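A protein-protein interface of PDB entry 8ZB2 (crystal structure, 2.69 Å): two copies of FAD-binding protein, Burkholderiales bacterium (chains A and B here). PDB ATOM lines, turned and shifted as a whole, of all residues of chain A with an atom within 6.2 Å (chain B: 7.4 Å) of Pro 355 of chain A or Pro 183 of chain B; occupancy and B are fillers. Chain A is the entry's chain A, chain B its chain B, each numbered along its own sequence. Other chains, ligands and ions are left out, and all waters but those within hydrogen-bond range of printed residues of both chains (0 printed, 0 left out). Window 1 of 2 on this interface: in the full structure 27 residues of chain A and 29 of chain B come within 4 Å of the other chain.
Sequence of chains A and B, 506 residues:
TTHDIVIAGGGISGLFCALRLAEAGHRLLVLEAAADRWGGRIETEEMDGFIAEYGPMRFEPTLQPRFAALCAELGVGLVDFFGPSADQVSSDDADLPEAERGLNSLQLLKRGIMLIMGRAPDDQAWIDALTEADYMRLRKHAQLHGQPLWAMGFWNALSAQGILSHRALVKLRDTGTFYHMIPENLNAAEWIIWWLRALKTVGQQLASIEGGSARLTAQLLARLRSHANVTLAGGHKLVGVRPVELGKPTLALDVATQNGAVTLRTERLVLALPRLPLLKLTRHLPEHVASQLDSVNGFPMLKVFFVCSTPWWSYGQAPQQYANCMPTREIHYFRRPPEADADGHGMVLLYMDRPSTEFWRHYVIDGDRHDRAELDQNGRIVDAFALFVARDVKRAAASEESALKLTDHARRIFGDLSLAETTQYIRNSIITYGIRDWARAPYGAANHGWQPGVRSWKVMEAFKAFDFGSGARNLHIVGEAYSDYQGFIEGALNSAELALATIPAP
Of the 13 printed residues of chain B, 4 touch a printed residue of chain A.
Printed residues of chain A that touch a printed residue of chain B: Arg 354, Pro 355, Glu 358 and Phe 359.
Among the printed residues, no Asp or Glu carboxylate lies within 4 Å of a Lys or Arg side-chain nitrogen of the other chain.
Arg 354 of chain A touches its own counterpart, Arg 354 of chain B.
Of the 7 pairs that touch across the chains among the printed residues, 1 has its exchanged pair printed and touching as well.
Pro 355 of chain A touches just these residues of chain B: Trp 155 (3.4 Å) and Pro 183 (3.6 Å).
Of the printed residues of chain B, Phe 359 of chain A touches Trp 155 and Asn 185.
Printed residues of chain A within 4 Å of Trp 155 of chain B: Pro 355 and Phe 359.
Pro 183 of chain B touches just these residues of chain A: Pro 355 (3.6 Å) and Glu 358 (3.4 Å).
Printed residues of chain A within 4 Å of Asn 185 of chain B: Glu 358 and Phe 359.
Arg 329 of chain B touches none of the printed residues of chain A.
Printed residues of chain A within 4 Å of Arg 354 of chain B: Arg 354.
The nearest residue of chain B that does not touch Pro 355 of chain A is Glu 184 of chain B (5.7 Å).
The nearest printed residue of chain B that does not touch Arg 354 of chain A is Glu 184 of chain B (5.5 Å).
Among the printed residues, merely in contact across the chains: Arg 354 of chain A with Arg 354 of chain B, Pro 355 of chain A with Trp 155 of chain B, Pro 355 of chain A with Pro 183 of chain B, Glu 358 of chain A with Pro 183 of chain B, Phe 359 of chain A with Trp 155 of chain B and Phe 359 of chain A with Asn 185 of chain B.
The guanidinium group (NH1) of Arg 354 of chain B lies within salt-bridge range of the side-chain carboxylate (OE1) of Glu 184 of chain B (3.2 Å).
The side-chain carboxylate (OE2) of Glu 358 of chain A is in salt-bridge range of the guanidinium group (NH1) of Arg 354 of chain A.
OG1 of Thr 357 of chain A is in hydrogen-bond range of OE2 of Glu 358 of chain A (3.3 Å).
The side-chain amide oxygen (OD1) of Asn 185 of chain B is in hydrogen-bond range of the backbone NH (N) of Trp 155 of chain B, 3.0 Å away.
ND2 of Asn 185 of chain B is in hydrogen-bond range of O of Glu 358 of chain A, 2.9 Å away.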
ATOM      1  N   ASP A 353      20.290  -2.721 -18.129  1.00  0.00           N
ATOM      2  CA  ASP A 353      19.945  -2.035 -19.399  1.00  0.00           C
ATOM      3  C   ASP A 353      18.573  -2.544 -19.841  1.00  0.00           C
ATOM      4  O   ASP A 353      17.910  -3.205 -19.051  1.00  0.00           O
ATOM      5  CB  ASP A 353      21.028  -2.244 -20.468  1.00  0.00           C
ATOM      6  CG  ASP A 353      21.238  -3.686 -20.882  1.00  0.00           C
ATOM      7  OD1 ASP A 353      20.591  -4.533 -20.291  1.00  0.00           O
ATOM      8  OD2 ASP A 353      22.057  -3.939 -21.794  1.00  0.00           O
ATOM      9  N   ARG A 354      18.150  -2.203 -21.053  1.00  0.00           N
ATOM     10  CA  ARG A 354      16.902  -2.727 -21.653  1.00  0.00           C
ATOM     11  C   ARG A 354      17.082  -4.240 -21.766  1.00  0.00           C
ATOM     12  O   ARG A 354      18.165  -4.692 -22.133  1.00  0.00           O
ATOM     13  CB  ARG A 354      16.674  -2.009 -22.986  1.00  0.00           C
ATOM     14  CG  ARG A 354      15.298  -2.230 -23.590  1.00  0.00           C
ATOM     15  CD  ARG A 354      15.133  -1.434 -24.876  1.00  0.00           C
ATOM     16  NE  ARG A 354      15.180   0.010 -24.677  1.00  0.00           N
ATOM     17  CZ  ARG A 354      14.217   0.730 -24.090  1.00  0.00           C
ATOM     18  NH1 ARG A 354      13.135   0.146 -23.597  1.00  0.00           N
ATOM     19  NH2 ARG A 354      14.343   2.043 -23.989  1.00  0.00           N
ATOM     20  N   PRO A 355      16.083  -5.084 -21.428  1.00  0.00           N
ATOM     21  CA  PRO A 355      14.742  -4.652 -21.030  1.00  0.00           C
ATOM     22  C   PRO A 355      14.442  -4.757 -19.523  1.00  0.00           C
ATOM     23  O   PRO A 355      13.324  -4.509 -19.109  1.00  0.00           O
ATOM     24  CB  PRO A 355      13.937  -5.716 -21.794  1.00  0.00           C
ATOM     25  CG  PRO A 355      14.737  -7.002 -21.553  1.00  0.00           C
ATOM     26  CD  PRO A 355      16.184  -6.553 -21.452  1.00  0.00           C
ATOM     27  N   SER A 356      15.440  -5.157 -18.738  1.00  0.00           N
ATOM     28  CA  SER A 356      15.354  -5.265 -17.266  1.00  0.00           C
ATOM     29  C   SER A 356      14.919  -3.907 -16.689  1.00  0.00           C
ATOM     30  O   SER A 356      14.093  -3.885 -15.743  1.00  0.00           O
ATOM     31  CB  SER A 356      16.674  -5.761 -16.735  1.00  0.00           C
ATOM     32  OG  SER A 356      17.482  -6.270 -17.812  1.00  0.00           O
ATOM     33  N   THR A 357      15.381  -2.800 -17.274  1.00  0.00           N
ATOM     34  CA  THR A 357      14.978  -1.418 -16.875  1.00  0.00           C
ATOM     35  C   THR A 357      13.452  -1.293 -16.744  1.00  0.00           C
ATOM     36  O   THR A 357      13.003  -0.667 -15.782  1.00  0.00           O
ATOM     37  CB  THR A 357      15.463  -0.369 -17.873  1.00  0.00           C
ATOM     38  OG1 THR A 357      15.142  -0.827 -19.182  1.00  0.00           O
ATOM     39  CG2 THR A 357      16.945  -0.109 -17.752  1.00  0.00           C
ATOM     40  N   GLU A 358      12.689  -1.881 -17.665  1.00  0.00           N
ATOM     41  CA  GLU A 358      11.202  -1.839 -17.678  1.00  0.00           C
ATOM     42  C   GLU A 358      10.615  -2.518 -16.444  1.00  0.00           C
ATOM     43  O   GLU A 358       9.515  -2.108 -16.044  1.00  0.00           O
ATOM     44  CB  GLU A 358      10.632  -2.543 -18.904  1.00  0.00           C
ATOM     45  CG  GLU A 358      11.115  -1.956 -20.214  1.00  0.00           C
ATOM     46  CD  GLU A 358      11.128  -0.443 -20.284  1.00  0.00           C
ATOM     47  OE1 GLU A 358      10.043   0.152 -20.199  1.00  0.00           O
ATOM     48  OE2 GLU A 358      12.237   0.131 -20.382  1.00  0.00           O
ATOM     49  N   PHE A 359      11.295  -3.520 -15.872  1.00  0.00           N
ATOM     50  CA  PHE A 359      10.809  -4.254 -14.669  1.00  0.00           C
ATOM     51  C   PHE A 359      10.732  -3.295 -13.481  1.00  0.00           C
ATOM     52  O   PHE A 359       9.705  -3.313 -12.768  1.00  0.00           O
ATOM     53  CB  PHE A 359      11.696  -5.449 -14.303  1.00  0.00           C
ATOM     54  CG  PHE A 359      11.180  -6.234 -13.119  1.00  0.00           C
ATOM     55  CD1 PHE A 359      11.563  -5.896 -11.828  1.00  0.00           C
ATOM     56  CD2 PHE A 359      10.296  -7.292 -13.293  1.00  0.00           C
ATOM     57  CE1 PHE A 359      11.075  -6.595 -10.737  1.00  0.00           C
ATOM     58  CE2 PHE A 359       9.797  -7.978 -12.200  1.00  0.00           C
ATOM     59  CZ  PHE A 359      10.191  -7.628 -10.929  1.00  0.00           C
ATOM     60  N   TRP B 155       4.761  -7.919 -16.195  1.00  0.00           N
ATOM     61  CA  TRP B 155       5.993  -8.663 -15.842  1.00  0.00           C
ATOM     62  C   TRP B 155       6.108  -8.786 -14.325  1.00  0.00           C
ATOM     63  O   TRP B 155       6.475  -9.859 -13.859  1.00  0.00           O
ATOM     64  CB  TRP B 155       7.205  -7.953 -16.438  1.00  0.00           C
ATOM     65  CG  TRP B 155       8.490  -8.703 -16.307  1.00  0.00           C
ATOM     66  CD1 TRP B 155       8.713  -9.860 -15.622  1.00  0.00           C
ATOM     67  CD2 TRP B 155       9.758  -8.313 -16.865  1.00  0.00           C
ATOM     68  NE1 TRP B 155      10.031 -10.214 -15.714  1.00  0.00           N
ATOM     69  CE2 TRP B 155      10.699  -9.290 -16.474  1.00  0.00           C
ATOM     70  CE3 TRP B 155      10.188  -7.229 -17.640  1.00  0.00           C
ATOM     71  CZ2 TRP B 155      12.043  -9.231 -16.857  1.00  0.00           C
ATOM     72  CZ3 TRP B 155      11.513  -7.157 -18.004  1.00  0.00           C
ATOM     73  CH2 TRP B 155      12.426  -8.150 -17.620  1.00  0.00           C
ATOM     74  N   ASP B 174      10.040 -15.494 -22.078  1.00  0.00           N
ATOM     75  CA  ASP B 174       9.796 -14.564 -23.209  1.00  0.00           C
ATOM     76  C   ASP B 174      10.669 -15.012 -24.386  1.00  0.00           C
ATOM     77  O   ASP B 174      10.329 -14.649 -25.521  1.00  0.00           O
ATOM     78  CB  ASP B 174      10.008 -13.092 -22.818  1.00  0.00           C
ATOM     79  CG  ASP B 174      11.377 -12.740 -22.253  1.00  0.00           C
ATOM     80  OD1 ASP B 174      11.440 -11.910 -21.306  1.00  0.00           O
ATOM     81  OD2 ASP B 174      12.375 -13.263 -22.779  1.00  0.00           O
ATOM     82  N   THR B 175      11.743 -15.769 -24.134  1.00  0.00           N
ATOM     83  CA  THR B 175      12.642 -16.334 -25.176  1.00  0.00           C
ATOM     84  C   THR B 175      11.890 -17.369 -26.039  1.00  0.00           C
ATOM     85  O   THR B 175      12.368 -17.604 -27.158  1.00  0.00           O
ATOM     86  CB  THR B 175      13.950 -16.873 -24.563  1.00  0.00           C
ATOM     87  OG1 THR B 175      13.792 -16.939 -23.147  1.00  0.00           O
ATOM     88  CG2 THR B 175      15.173 -16.033 -24.875  1.00  0.00           C
ATOM     89  N   HIS B 180       3.685 -11.356 -26.094  1.00  0.00           N
ATOM     90  CA  HIS B 180       3.049 -11.295 -24.756  1.00  0.00           C
ATOM     91  C   HIS B 180       3.497 -10.024 -24.024  1.00  0.00           C
ATOM     92  O   HIS B 180       2.946  -9.764 -22.947  1.00  0.00           O
ATOM     93  CB  HIS B 180       3.469 -12.551 -23.994  1.00  0.00           C
ATOM     94  CG  HIS B 180       4.919 -12.817 -24.218  1.00  0.00           C
ATOM     95  ND1 HIS B 180       5.381 -13.799 -25.071  1.00  0.00           N
ATOM     96  CD2 HIS B 180       6.005 -12.126 -23.810  1.00  0.00           C
ATOM     97  CE1 HIS B 180       6.700 -13.748 -25.109  1.00  0.00           C
ATOM     98  NE2 HIS B 180       7.105 -12.731 -24.344  1.00  0.00           N
ATOM     99  N   MET B 181       4.513  -9.323 -24.559  1.00  0.00           N
ATOM    100  CA  MET B 181       4.935  -7.948 -24.162  1.00  0.00           C
ATOM    101  C   MET B 181       5.264  -7.943 -22.660  1.00  0.00           C
ATOM    102  O   MET B 181       4.706  -7.155 -21.857  1.00  0.00           O
ATOM    103  CB  MET B 181       3.845  -6.939 -24.544  1.00  0.00           C
ATOM    104  CG  MET B 181       4.012  -6.313 -25.947  1.00  0.00           C
ATOM    105  SD  MET B 181       4.380  -7.449 -27.306  1.00  0.00           S
ATOM    106  CE  MET B 181       5.801  -6.634 -28.040  1.00  0.00           C
ATOM    107  N   ILE B 182       6.147  -8.865 -22.311  1.00  0.00           N
ATOM    108  CA  ILE B 182       6.768  -9.020 -20.969  1.00  0.00           C
ATOM    109  C   ILE B 182       7.905  -8.006 -20.887  1.00  0.00           C
ATOM    110  O   ILE B 182       7.820  -7.115 -20.051  1.00  0.00           O
ATOM    111  CB  ILE B 182       7.150 -10.503 -20.718  1.00  0.00           C
ATOM    112  CG1 ILE B 182       5.938 -11.250 -20.152  1.00  0.00           C
ATOM    113  CG2 ILE B 182       8.373 -10.675 -19.828  1.00  0.00           C
ATOM    114  CD1 ILE B 182       6.014 -12.749 -20.263  1.00  0.00           C
ATOM    115  N   PRO B 183       8.943  -8.044 -21.764  1.00  0.00           N
ATOM    116  CA  PRO B 183      10.000  -7.025 -21.753  1.00  0.00           C
ATOM    117  C   PRO B 183       9.573  -5.577 -22.068  1.00  0.00           C
ATOM    118  O   PRO B 183      10.424  -4.712 -22.020  1.00  0.00           O
ATOM    119  CB  PRO B 183      11.006  -7.487 -22.826  1.00  0.00           C
ATOM    120  CG  PRO B 183      10.264  -8.507 -23.668  1.00  0.00           C
ATOM    121  CD  PRO B 183       9.198  -9.096 -22.769  1.00  0.00           C
ATOM    122  N   GLU B 184       8.309  -5.350 -22.429  1.00  0.00           N
ATOM    123  CA  GLU B 184       7.713  -3.998 -22.587  1.00  0.00           C
ATOM    124  C   GLU B 184       6.944  -3.680 -21.310  1.00  0.00           C
ATOM    125  O   GLU B 184       6.539  -2.542 -21.118  1.00  0.00           O
ATOM    126  CB  GLU B 184       6.805  -3.938 -23.818  1.00  0.00           C
ATOM    127  CG  GLU B 184       7.403  -4.519 -25.104  1.00  0.00           C
ATOM    128  CD  GLU B 184       8.789  -4.035 -25.532  1.00  0.00           C
ATOM    129  OE1 GLU B 184       8.999  -2.786 -25.622  1.00  0.00           O
ATOM    130  OE2 GLU B 184       9.668  -4.912 -25.784  1.00  0.00           O
ATOM    131  N   ASN B 185       6.760  -4.679 -20.469  1.00  0.00           N
ATOM    132  CA  ASN B 185       6.135  -4.576 -19.133  1.00  0.00           C
ATOM    133  C   ASN B 185       4.922  -3.651 -19.195  1.00  0.00           C
ATOM    134  O   ASN B 185       4.982  -2.561 -18.611  1.00  0.00           O
ATOM    135  CB  ASN B 185       7.147  -4.169 -18.064  1.00  0.00           C
ATOM    136  CG  ASN B 185       6.630  -4.464 -16.671  1.00  0.00           C
ATOM    137  OD1 ASN B 185       5.549  -5.040 -16.530  1.00  0.00           O
ATOM    138  ND2 ASN B 185       7.389  -4.092 -15.648  1.00  0.00           N
ATOM    139  N   LEU B 186       3.847  -4.109 -19.832  1.00  0.00           N
ATOM    140  CA  LEU B 186       2.589  -3.343 -19.997  1.00  0.00           C
ATOM    141  C   LEU B 186       1.749  -3.429 -18.723  1.00  0.00           C
ATOM    142  O   LEU B 186       2.083  -4.210 -17.815  1.00  0.00           O
ATOM    143  CB  LEU B 186       1.793  -3.890 -21.187  1.00  0.00           C
ATOM    144  CG  LEU B 186       2.533  -3.922 -22.522  1.00  0.00           C
ATOM    145  CD1 LEU B 186       1.613  -4.395 -23.634  1.00  0.00           C
ATOM    146  CD2 LEU B 186       3.110  -2.567 -22.873  1.00  0.00           C
ATOM    147  N   ARG B 329      11.999 -12.647 -35.074  1.00  0.00           N
ATOM    148  CA  ARG B 329      11.307 -13.435 -34.028  1.00  0.00           C
ATOM    149  C   ARG B 329      10.684 -14.661 -34.715  1.00  0.00           C
ATOM    150  O   ARG B 329      11.197 -15.774 -34.547  1.00  0.00           O
ATOM    151  CB  ARG B 329      10.291 -12.581 -33.272  1.00  0.00           C
ATOM    152  CG  ARG B 329       9.287 -13.378 -32.440  1.00  0.00           C
ATOM    153  CD  ARG B 329       9.394 -13.282 -30.922  1.00  0.00           C
ATOM    154  NE  ARG B 329      10.780 -13.102 -30.500  1.00  0.00           N
ATOM    155  CZ  ARG B 329      11.184 -12.499 -29.386  1.00  0.00           C
ATOM    156  NH1 ARG B 329      10.309 -12.018 -28.511  1.00  0.00           N
ATOM    157  NH2 ARG B 329      12.483 -12.394 -29.155  1.00  0.00           N
ATOM    158  N   ASP B 353       9.952  -8.183 -33.766  1.00  0.00           N
ATOM    159  CA  ASP B 353       9.734  -7.139 -32.726  1.00  0.00           C
ATOM    160  C   ASP B 353      11.104  -6.633 -32.273  1.00  0.00           C
ATOM    161  O   ASP B 353      12.104  -6.962 -32.918  1.00  0.00           O
ATOM    162  CB  ASP B 353       8.905  -7.674 -31.555  1.00  0.00           C
ATOM    163  CG  ASP B 353       9.535  -8.848 -30.821  1.00  0.00           C
ATOM    164  OD1 ASP B 353      10.645  -9.275 -31.239  1.00  0.00           O
ATOM    165  OD2 ASP B 353       8.898  -9.344 -29.846  1.00  0.00           O
ATOM    166  N   ARG B 354      11.150  -5.827 -31.219  1.00  0.00           N
ATOM    167  CA  ARG B 354      12.428  -5.363 -30.622  1.00  0.00           C
ATOM    168  C   ARG B 354      13.134  -6.619 -30.117  1.00  0.00           C
ATOM    169  O   ARG B 354      12.476  -7.488 -29.559  1.00  0.00           O
ATOM    170  CB  ARG B 354      12.148  -4.311 -29.540  1.00  0.00           C
ATOM    171  CG  ARG B 354      13.387  -3.537 -29.110  1.00  0.00           C
ATOM    172  CD  ARG B 354      13.285  -2.639 -27.893  1.00  0.00           C
ATOM    173  NE  ARG B 354      12.782  -1.338 -28.305  1.00  0.00           N
ATOM    174  CZ  ARG B 354      11.495  -1.043 -28.488  1.00  0.00           C
ATOM    175  NH1 ARG B 354      10.557  -1.955 -28.270  1.00  0.00           N
ATOM    176  NH2 ARG B 354      11.146   0.174 -28.869  1.00  0.00           N
